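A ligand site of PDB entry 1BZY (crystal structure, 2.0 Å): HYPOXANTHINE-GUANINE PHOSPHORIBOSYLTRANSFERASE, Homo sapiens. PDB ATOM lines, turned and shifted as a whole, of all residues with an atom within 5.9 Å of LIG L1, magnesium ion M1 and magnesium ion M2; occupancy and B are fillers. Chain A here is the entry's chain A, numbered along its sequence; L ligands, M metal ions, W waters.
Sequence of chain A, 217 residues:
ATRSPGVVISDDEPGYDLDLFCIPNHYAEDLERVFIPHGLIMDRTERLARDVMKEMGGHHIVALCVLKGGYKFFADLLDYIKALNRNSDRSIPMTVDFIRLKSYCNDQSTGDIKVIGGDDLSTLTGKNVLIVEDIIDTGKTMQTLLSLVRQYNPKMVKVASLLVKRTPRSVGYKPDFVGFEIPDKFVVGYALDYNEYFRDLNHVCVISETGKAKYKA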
ATOM      1  N   VAL A  66      17.604  20.862  10.310  1.00  0.00           N
ATOM      2  CA  VAL A  66      19.005  21.112   9.970  1.00  0.00           C
ATOM      3  C   VAL A  66      19.215  20.599   8.551  1.00  0.00           C
ATOM      4  O   VAL A  66      19.320  19.386   8.327  1.00  0.00           O
ATOM      5  CB  VAL A  66      19.951  20.372  10.926  1.00  0.00           C
ATOM      6  CG1 VAL A  66      21.396  20.756  10.649  1.00  0.00           C
ATOM      7  CG2 VAL A  66      19.580  20.680  12.361  1.00  0.00           C
ATOM      8  N   LEU A  67      19.268  21.520   7.598  1.00  0.00           N
ATOM      9  CA  LEU A  67      19.429  21.203   6.181  1.00  0.00           C
ATOM     10  C   LEU A  67      20.897  20.916   5.851  1.00  0.00           C
ATOM     11  O   LEU A  67      21.796  21.419   6.532  1.00  0.00           O
ATOM     12  CB  LEU A  67      18.930  22.399   5.350  1.00  0.00           C
ATOM     13  CG  LEU A  67      17.576  22.423   4.615  1.00  0.00           C
ATOM     14  CD1 LEU A  67      16.717  21.245   4.977  1.00  0.00           C
ATOM     15  CD2 LEU A  67      16.885  23.736   4.916  1.00  0.00           C
ATOM     16  N   LYS A  68      21.162  20.124   4.815  1.00  0.00           N
ATOM     17  CA  LYS A  68      20.135  19.507   3.976  1.00  0.00           C
ATOM     18  C   LYS A  68      19.886  18.093   4.481  1.00  0.00           C
ATOM     19  O   LYS A  68      18.818  17.527   4.231  1.00  0.00           O
ATOM     20  CB  LYS A  68      20.617  19.377   2.532  1.00  0.00           C
ATOM     21  CG  LYS A  68      20.880  20.661   1.775  1.00  0.00           C
ATOM     22  CD  LYS A  68      21.267  20.319   0.337  1.00  0.00           C
ATOM     23  CE  LYS A  68      21.965  21.480  -0.358  1.00  0.00           C
ATOM     24  NZ  LYS A  68      22.553  21.086  -1.661  1.00  0.00           N
ATOM     25  N   GLY A  69      20.882  17.530   5.157  1.00  0.00           N
ATOM     26  CA  GLY A  69      20.811  16.169   5.643  1.00  0.00           C
ATOM     27  C   GLY A  69      19.595  15.692   6.403  1.00  0.00           C
ATOM     28  O   GLY A  69      19.134  14.584   6.176  1.00  0.00           O
ATOM     29  N   GLY A  70      19.072  16.503   7.313  1.00  0.00           N
ATOM     30  CA  GLY A  70      17.915  16.083   8.069  1.00  0.00           C
ATOM     31  C   GLY A  70      16.554  16.312   7.440  1.00  0.00           C
ATOM     32  O   GLY A  70      15.551  16.120   8.123  1.00  0.00           O
ATOM     33  N   ARG A 100      20.483  25.899   7.502  1.00  0.00           N
ATOM     34  CA  ARG A 100      21.435  25.110   6.750  1.00  0.00           C
ATOM     35  C   ARG A 100      22.851  25.310   7.279  1.00  0.00           C
ATOM     36  O   ARG A 100      23.326  26.431   7.373  1.00  0.00           O
ATOM     37  CB  ARG A 100      21.384  25.462   5.262  1.00  0.00           C
ATOM     38  CG  ARG A 100      22.648  25.102   4.482  1.00  0.00           C
ATOM     39  CD  ARG A 100      22.418  24.005   3.462  1.00  0.00           C
ATOM     40  NE  ARG A 100      22.661  24.459   2.102  1.00  0.00           N
ATOM     41  CZ  ARG A 100      23.719  24.114   1.377  1.00  0.00           C
ATOM     42  NH1 ARG A 100      24.636  23.308   1.861  1.00  0.00           N
ATOM     43  NH2 ARG A 100      23.853  24.590   0.144  1.00  0.00           N
ATOM     44  N   LEU A 101      23.486  24.204   7.630  1.00  0.00           N
ATOM     45  CA  LEU A 101      24.858  24.215   8.115  1.00  0.00           C
ATOM     46  C   LEU A 101      25.644  23.297   7.173  1.00  0.00           C
ATOM     47  O   LEU A 101      25.120  22.266   6.741  1.00  0.00           O
ATOM     48  CB  LEU A 101      24.916  23.676   9.546  1.00  0.00           C
ATOM     49  CG  LEU A 101      24.849  24.655  10.725  1.00  0.00           C
ATOM     50  CD1 LEU A 101      23.910  25.799  10.404  1.00  0.00           C
ATOM     51  CD2 LEU A 101      24.364  23.915  11.974  1.00  0.00           C
ATOM     52  N   LYS A 102      26.868  23.670   6.842  1.00  0.00           N
ATOM     53  CA  LYS A 102      27.684  22.857   5.946  1.00  0.00           C
ATOM     54  C   LYS A 102      29.105  22.745   6.459  1.00  0.00           C
ATOM     55  O   LYS A 102      29.703  23.740   6.885  1.00  0.00           O
ATOM     56  CB  LYS A 102      27.689  23.454   4.543  1.00  0.00           C
ATOM     57  CG  LYS A 102      28.362  22.584   3.497  1.00  0.00           C
ATOM     58  CD  LYS A 102      28.349  23.244   2.133  1.00  0.00           C
ATOM     59  CE  LYS A 102      29.037  22.366   1.101  1.00  0.00           C
ATOM     60  NZ  LYS A 102      28.085  21.425   0.439  1.00  0.00           N
ATOM     61  N   SER A 103      29.670  21.536   6.421  1.00  0.00           N
ATOM     62  CA  SER A 103      31.026  21.344   6.909  1.00  0.00           C
ATOM     63  C   SER A 103      31.785  20.118   6.376  1.00  0.00           C
ATOM     64  O   SER A 103      32.976  19.957   6.625  1.00  0.00           O
ATOM     65  CB  SER A 103      31.017  21.307   8.448  1.00  0.00           C
ATOM     66  OG  SER A 103      30.346  20.155   8.940  1.00  0.00           O
ATOM     67  N   TYR A 104      31.096  19.263   5.618  1.00  0.00           N
ATOM     68  CA  TYR A 104      31.747  18.058   5.098  1.00  0.00           C
ATOM     69  C   TYR A 104      32.219  18.113   3.662  1.00  0.00           C
ATOM     70  O   TYR A 104      31.623  18.790   2.829  1.00  0.00           O
ATOM     71  CB  TYR A 104      30.824  16.841   5.265  1.00  0.00           C
ATOM     72  CG  TYR A 104      31.015  16.149   6.595  1.00  0.00           C
ATOM     73  CD1 TYR A 104      30.687  16.795   7.782  1.00  0.00           C
ATOM     74  CD2 TYR A 104      31.534  14.862   6.657  1.00  0.00           C
ATOM     75  CE1 TYR A 104      30.870  16.168   9.007  1.00  0.00           C
ATOM     76  CE2 TYR A 104      31.710  14.228   7.893  1.00  0.00           C
ATOM     77  CZ  TYR A 104      31.381  14.884   9.058  1.00  0.00           C
ATOM     78  OH  TYR A 104      31.552  14.276  10.278  1.00  0.00           O
ATOM     79  N   GLU A 133      17.913  16.592  13.345  1.00  0.00           N
ATOM     80  CA  GLU A 133      19.122  16.396  12.560  1.00  0.00           C
ATOM     81  C   GLU A 133      19.280  14.968  12.053  1.00  0.00           C
ATOM     82  O   GLU A 133      18.638  14.048  12.559  1.00  0.00           O
ATOM     83  CB  GLU A 133      20.328  16.786  13.430  1.00  0.00           C
ATOM     84  CG  GLU A 133      21.683  16.395  12.901  1.00  0.00           C
ATOM     85  CD  GLU A 133      22.095  17.185  11.686  1.00  0.00           C
ATOM     86  OE1 GLU A 133      21.337  17.177  10.699  1.00  0.00           O
ATOM     87  OE2 GLU A 133      23.175  17.828  11.720  1.00  0.00           O
ATOM     88  N   ASP A 134      20.125  14.774  11.041  1.00  0.00           N
ATOM     89  CA  ASP A 134      20.340  13.457  10.470  1.00  0.00           C
ATOM     90  C   ASP A 134      21.288  12.582  11.266  1.00  0.00           C
ATOM     91  O   ASP A 134      20.976  11.423  11.566  1.00  0.00           O
ATOM     92  CB  ASP A 134      20.818  13.553   9.007  1.00  0.00           C
ATOM     93  CG  ASP A 134      22.064  14.439   8.843  1.00  0.00           C
ATOM     94  OD1 ASP A 134      22.591  14.960   9.856  1.00  0.00           O
ATOM     95  OD2 ASP A 134      22.503  14.627   7.697  1.00  0.00           O
ATOM     96  N   THR A 141      28.914  20.030  14.446  1.00  0.00           N
ATOM     97  CA  THR A 141      27.741  20.707  13.914  1.00  0.00           C
ATOM     98  C   THR A 141      26.684  21.037  14.969  1.00  0.00           C
ATOM     99  O   THR A 141      26.241  22.175  15.065  1.00  0.00           O
ATOM    100  CB  THR A 141      27.074  19.863  12.819  1.00  0.00           C
ATOM    101  OG1 THR A 141      27.967  19.746  11.697  1.00  0.00           O
ATOM    102  CG2 THR A 141      25.778  20.516  12.349  1.00  0.00           C
ATOM    103  N   PHE A 186      30.707   5.714   7.024  1.00  0.00           N
ATOM    104  CA  PHE A 186      30.082   6.866   6.381  1.00  0.00           C
ATOM    105  C   PHE A 186      28.878   6.422   5.572  1.00  0.00           C
ATOM    106  O   PHE A 186      29.004   6.022   4.410  1.00  0.00           O
ATOM    107  CB  PHE A 186      31.082   7.604   5.479  1.00  0.00           C
ATOM    108  CG  PHE A 186      30.649   9.011   5.140  1.00  0.00           C
ATOM    109  CD1 PHE A 186      30.923  10.065   6.008  1.00  0.00           C
ATOM    110  CD2 PHE A 186      29.933   9.267   3.979  1.00  0.00           C
ATOM    111  CE1 PHE A 186      30.492  11.357   5.721  1.00  0.00           C
ATOM    112  CE2 PHE A 186      29.495  10.562   3.679  1.00  0.00           C
ATOM    113  CZ  PHE A 186      29.776  11.613   4.560  1.00  0.00           C
ATOM    114  N   ALA A 191      18.368  11.244   2.524  1.00  0.00           N
ATOM    115  CA  ALA A 191      18.799  12.647   2.562  1.00  0.00           C
ATOM    116  C   ALA A 191      20.266  12.835   2.936  1.00  0.00           C
ATOM    117  O   ALA A 191      20.815  13.942   2.765  1.00  0.00           O
ATOM    118  CB  ALA A 191      17.908  13.454   3.512  1.00  0.00           C
ATOM    119  N   LEU A 192      20.905  11.781   3.462  1.00  0.00           N
ATOM    120  CA  LEU A 192      22.328  11.854   3.830  1.00  0.00           C
ATOM    121  C   LEU A 192      23.121  11.629   2.542  1.00  0.00           C
ATOM    122  O   LEU A 192      22.947  10.614   1.862  1.00  0.00           O
ATOM    123  CB  LEU A 192      22.682  10.794   4.875  1.00  0.00           C
ATOM    124  CG  LEU A 192      22.316  11.068   6.348  1.00  0.00           C
ATOM    125  CD1 LEU A 192      20.903  10.567   6.598  1.00  0.00           C
ATOM    126  CD2 LEU A 192      23.288  10.344   7.284  1.00  0.00           C
ATOM    127  N   ASP A 193      23.988  12.582   2.230  1.00  0.00           N
ATOM    128  CA  ASP A 193      24.759  12.553   0.987  1.00  0.00           C
ATOM    129  C   ASP A 193      26.260  12.293   1.116  1.00  0.00           C
ATOM    130  O   ASP A 193      26.826  12.194   2.201  1.00  0.00           O
ATOM    131  CB  ASP A 193      24.618  13.893   0.275  1.00  0.00           C
ATOM    132  CG  ASP A 193      25.488  14.966   0.913  1.00  0.00           C
ATOM    133  OD1 ASP A 193      25.431  15.093   2.152  1.00  0.00           O
ATOM    134  OD2 ASP A 193      26.249  15.672   0.204  1.00  0.00           O
ATOM    135  N   TYR A 194      26.864  12.208  -0.066  1.00  0.00           N
ATOM    136  CA  TYR A 194      28.295  12.055  -0.239  1.00  0.00           C
ATOM    137  C   TYR A 194      28.520  13.025  -1.406  1.00  0.00           C
ATOM    138  O   TYR A 194      28.257  12.692  -2.564  1.00  0.00           O
ATOM    139  CB  TYR A 194      28.669  10.643  -0.663  1.00  0.00           C
ATOM    140  CG  TYR A 194      30.146  10.494  -0.975  1.00  0.00           C
ATOM    141  CD1 TYR A 194      31.091  10.471   0.049  1.00  0.00           C
ATOM    142  CD2 TYR A 194      30.585  10.380  -2.294  1.00  0.00           C
ATOM    143  CE1 TYR A 194      32.460  10.334  -0.226  1.00  0.00           C
ATOM    144  CE2 TYR A 194      31.951  10.255  -2.582  1.00  0.00           C
ATOM    145  CZ  TYR A 194      32.877  10.222  -1.548  1.00  0.00           C
ATOM    146  OH  TYR A 194      34.211  10.082  -1.837  1.00  0.00           O
ATOM    147  N   ASN A 195      28.954  14.244  -1.079  1.00  0.00           N
ATOM    148  CA  ASN A 195      29.172  15.256  -2.100  1.00  0.00           C
ATOM    149  C   ASN A 195      27.908  15.500  -2.914  1.00  0.00           C
ATOM    150  O   ASN A 195      27.945  15.564  -4.137  1.00  0.00           O
ATOM    151  CB  ASN A 195      30.299  14.847  -3.041  1.00  0.00           C
ATOM    152  CG  ASN A 195      31.625  14.708  -2.330  1.00  0.00           C
ATOM    153  OD1 ASN A 195      31.982  15.521  -1.470  1.00  0.00           O
ATOM    154  ND2 ASN A 195      32.376  13.671  -2.683  1.00  0.00           N
ATOM    155  N   GLU A 196      26.785  15.635  -2.200  1.00  0.00           N
ATOM    156  CA  GLU A 196      25.465  15.889  -2.788  1.00  0.00           C
ATOM    157  C   GLU A 196      24.780  14.688  -3.434  1.00  0.00           C
ATOM    158  O   GLU A 196      23.599  14.760  -3.799  1.00  0.00           O
ATOM    159  CB  GLU A 196      25.538  17.042  -3.790  1.00  0.00           C
ATOM    160  CG  GLU A 196      25.987  18.374  -3.174  1.00  0.00           C
ATOM    161  CD  GLU A 196      25.179  18.743  -1.964  1.00  0.00           C
ATOM    162  OE1 GLU A 196      23.969  18.460  -1.933  1.00  0.00           O
ATOM    163  OE2 GLU A 196      25.757  19.343  -1.020  1.00  0.00           O
ATOM    164  N   ARG A 199      21.241  11.482  -1.894  1.00  0.00           N
ATOM    165  CA  ARG A 199      20.140  12.036  -1.108  1.00  0.00           C
ATOM    166  C   ARG A 199      18.834  11.415  -1.612  1.00  0.00           C
ATOM    167  O   ARG A 199      17.919  11.131  -0.831  1.00  0.00           O
ATOM    168  CB  ARG A 199      20.091  13.552  -1.278  1.00  0.00           C
ATOM    169  CG  ARG A 199      21.314  14.263  -0.749  1.00  0.00           C
ATOM    170  CD  ARG A 199      20.928  15.566  -0.083  1.00  0.00           C
ATOM    171  NE  ARG A 199      22.053  16.482   0.000  1.00  0.00           N
ATOM    172  CZ  ARG A 199      22.735  16.704   1.114  1.00  0.00           C
ATOM    173  NH1 ARG A 199      22.409  16.065   2.241  1.00  0.00           N
ATOM    174  NH2 ARG A 199      23.768  17.548   1.096  1.00  0.00           N
HETATM  175  P1  LIG L   1      24.446  18.502   4.360  1.00  0.00           P
HETATM  176  O1  LIG L   1      23.864  19.596   3.527  1.00  0.00           O
HETATM  177  O2  LIG L   1      23.552  18.162   5.644  1.00  0.00           O
HETATM  178  O3  LIG L   1      24.597  17.282   3.540  1.00  0.00           O
HETATM  179  O4  LIG L   1      25.799  19.030   4.937  1.00  0.00           O
HETATM  180  P2  LIG L   1      26.949  18.454   5.847  1.00  0.00           P
HETATM  181  O5  LIG L   1      27.268  17.087   5.419  1.00  0.00           O
HETATM  182  O6  LIG L   1      26.559  18.489   7.267  1.00  0.00           O
HETATM  183  O7  LIG L   1      28.156  19.447   5.558  1.00  0.00           O
HETATM  184  P1  LG2 L   2      29.504  16.531  12.759  1.00  0.00           P
HETATM  185  C1  LG2 L   2      26.586  11.363   5.784  1.00  0.00           C
HETATM  186  O1  LG2 L   2      28.798  15.942  13.915  1.00  0.00           O
HETATM  187  O2  LG2 L   2      29.684  17.988  12.841  1.00  0.00           O
HETATM  188  O3  LG2 L   2      30.782  15.804  12.526  1.00  0.00           O
HETATM  189  O4  LG2 L   2      28.726  16.153  11.498  1.00  0.00           O
HETATM  190  C2  LG2 L   2      27.330  15.992  11.363  1.00  0.00           C
HETATM  191  C3  LG2 L   2      26.951  16.630  10.093  1.00  0.00           C
HETATM  192  N1  LG2 L   2      27.735  16.114   9.018  1.00  0.00           N
HETATM  193  C4  LG2 L   2      25.513  16.377   9.836  1.00  0.00           C
HETATM  194  O5  LG2 L   2      24.909  17.635   9.544  1.00  0.00           O
HETATM  195  C5  LG2 L   2      25.542  15.423   8.679  1.00  0.00           C
HETATM  196  O6  LG2 L   2      24.659  15.820   7.637  1.00  0.00           O
HETATM  197  C6  LG2 L   2      26.994  15.301   8.124  1.00  0.00           C
HETATM  198  C7  LG2 L   2      27.470  13.853   8.322  1.00  0.00           C
HETATM  199  C8  LG2 L   2      28.218  13.369   9.414  1.00  0.00           C
HETATM  200  N2  LG2 L   2      28.506  12.098   9.385  1.00  0.00           N
HETATM  201  C9  LG2 L   2      27.908  11.650   8.198  1.00  0.00           C
HETATM  202  C10 LG2 L   2      27.884  10.318   7.642  1.00  0.00           C
HETATM  203  O7  LG2 L   2      28.384   9.311   8.123  1.00  0.00           O
HETATM  204  N3  LG2 L   2      27.193  10.257   6.418  1.00  0.00           N
HETATM  205  N4  LG2 L   2      25.966  11.144   4.616  1.00  0.00           N
HETATM  206  N5  LG2 L   2      26.606  12.624   6.321  1.00  0.00           N
HETATM  207  C11 LG2 L   2      27.278  12.708   7.530  1.00  0.00           C
HETATM  208 MG    MG M   1      24.096  18.054   7.658  1.00  0.00          MG
HETATM  209 MG    MG M   2      26.384  16.030   3.815  1.00  0.00          MG
HETATM  210  O   HOH W   1      24.066  20.208   7.951  1.00  0.00           O
HETATM  211  O   HOH W   2      27.665  20.336   9.044  1.00  0.00           O
HETATM  212  O   HOH W   3      27.682  17.085   2.269  1.00  0.00           O
HETATM  213  O   HOH W   4      27.752  14.456   3.823  1.00  0.00           O
HETATM  214  O   HOH W   5      25.308  20.618   1.289  1.00  0.00           O
HETATM  215  O   HOH W   6      24.702  22.004   4.071  1.00  0.00           O
HETATM  216  O   HOH W   7      28.870  19.254   2.844  1.00  0.00           O
HETATM  217  O   HOH W   8      21.935  17.996   8.141  1.00  0.00           O
HETATM  218  O   HOH W   9      25.256  14.564   5.035  1.00  0.00           O
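Of the 21 residues printed, 1 comes within 4 Å of magnesium ion M2. The nearest printed residue that does not touch magnesium ion M2 is Arg 199 (4.1 Å).
Water W4 binds magnesium ion M2, 2.1 Å away. O5 of LIG L1 is bound to magnesium ion M2 (2.1 Å). Magnesium ion M2 is bound by OD1 of Asp 193, at 2.1 Å. O3 of LIG L1 binds magnesium ion M2, 2.2 Å away. Magnesium ion M2 is bound by water W9, at 2.2 Å. Water W3 is bound to magnesium ion M2, 2.3 Å away.
Magnesium ion M1 is bound by an oxygen (O2) of LIG L1, an oxygen (O5) of LG2 L2, water W1, water W8, an oxygen (O6) of LG2 L2 and an oxygen (O6) of LIG L1.
Asp 134 touches magnesium ion M1.
Water W1 bridges O of Leu 101 and O of Leu 67. Water W4 lies within hydrogen-bond range of O of Asp 193 (2.9 Å) and N5 of LG2 L2 (3.3 Å). Water W6 lies within hydrogen-bond range of the guanidinium group of Arg 100 (2.6 Å), an oxygen (O1) of LIG L1 (2.6 Å) and the backbone carbonyl oxygen of Leu 101 (2.7 Å). Water W2 bridges OG of Ser 103 (2.7 Å) and OG1 of Thr 141 (2.7 Å). Water W7 lies within hydrogen-bond range of the backbone carbonyl oxygen (O) of Tyr 104 (2.8 Å), an oxygen (O7) of LIG L1 (2.8 Å) and the side-chain amino group (NZ) of Lys 102 (3.3 Å).
The guanidinium group (NH2) of Arg 199 is in salt-bridge range of an oxygen (O1) of LIG L1 (3.2 Å). N of Gly 69 sits close to O2 of LIG L1. N of Ser 103 sits at hydrogen-bond distance from O7 of LIG L1, at 2.7 Å. N of Tyr 104 is in hydrogen-bond range of O7 of LIG L1 (2.9 Å). An oxygen (O2) of LG2 L2 lies within hydrogen-bond range of the side-chain hydroxyl (OG1) of Thr 141. The backbone NH (N) of Thr 141 lies within hydrogen-bond range of an oxygen (O2) of LG2 L2. The side-chain carboxylate (OE2) of Glu 133 lies close to an oxygen (O5) of LG2 L2, 2.8 Å away. O6 of LG2 L2 lies close to OD2 of Asp 134 (2.5 Å). O1 of LIG L1 lies within hydrogen-bond range of N of Lys 68 (3.0 Å). OH of Tyr 104 is in hydrogen-bond range of O3 of LG2 L2 (2.8 Å). A nitrogen (N4) of LG2 L2 lies within hydrogen-bond range of the backbone carbonyl oxygen of Asp 193 (2.8 Å).
The backbone carbonyl oxygen of Leu 67 sits at hydrogen-bond distance from the backbone NH of Leu 101, at 3.4 Å. The side-chain amino group (NZ) of Lys 68 is in salt-bridge range of the side-chain carboxylate (OE1) of Glu 196 (3.0 Å). The guanidinium group (NH2) of Arg 199 lies within salt-bridge range of the side-chain carboxylate (OE1) of Glu 196 (3.2 Å). NZ of Lys 102 is in salt-bridge range of OE2 of Glu 196 (3.4 Å). The backbone NH of Glu 196 lies within hydrogen-bond range of the side-chain carboxylate of Asp 193, 2.5 Å away. The side-chain carboxylate of Asp 193 is in salt-bridge range of the guanidinium group of Arg 199, at 3.2 Å. The side-chain carboxylate (OD1) of Asp 134 lies close to the side-chain carboxylate (OE1) of Glu 133 (2.7 Å). O of Ala 191 sits at hydrogen-bond distance from NH1 of Arg 199, 2.7 Å away.
Merely in contact with LIG L1: Leu 67 (3.8 Å), Leu 101 (3.8 Å) and Lys 102 (3.5 Å). Of the 21 residues printed, 9 come within 4 Å of LIG L1.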
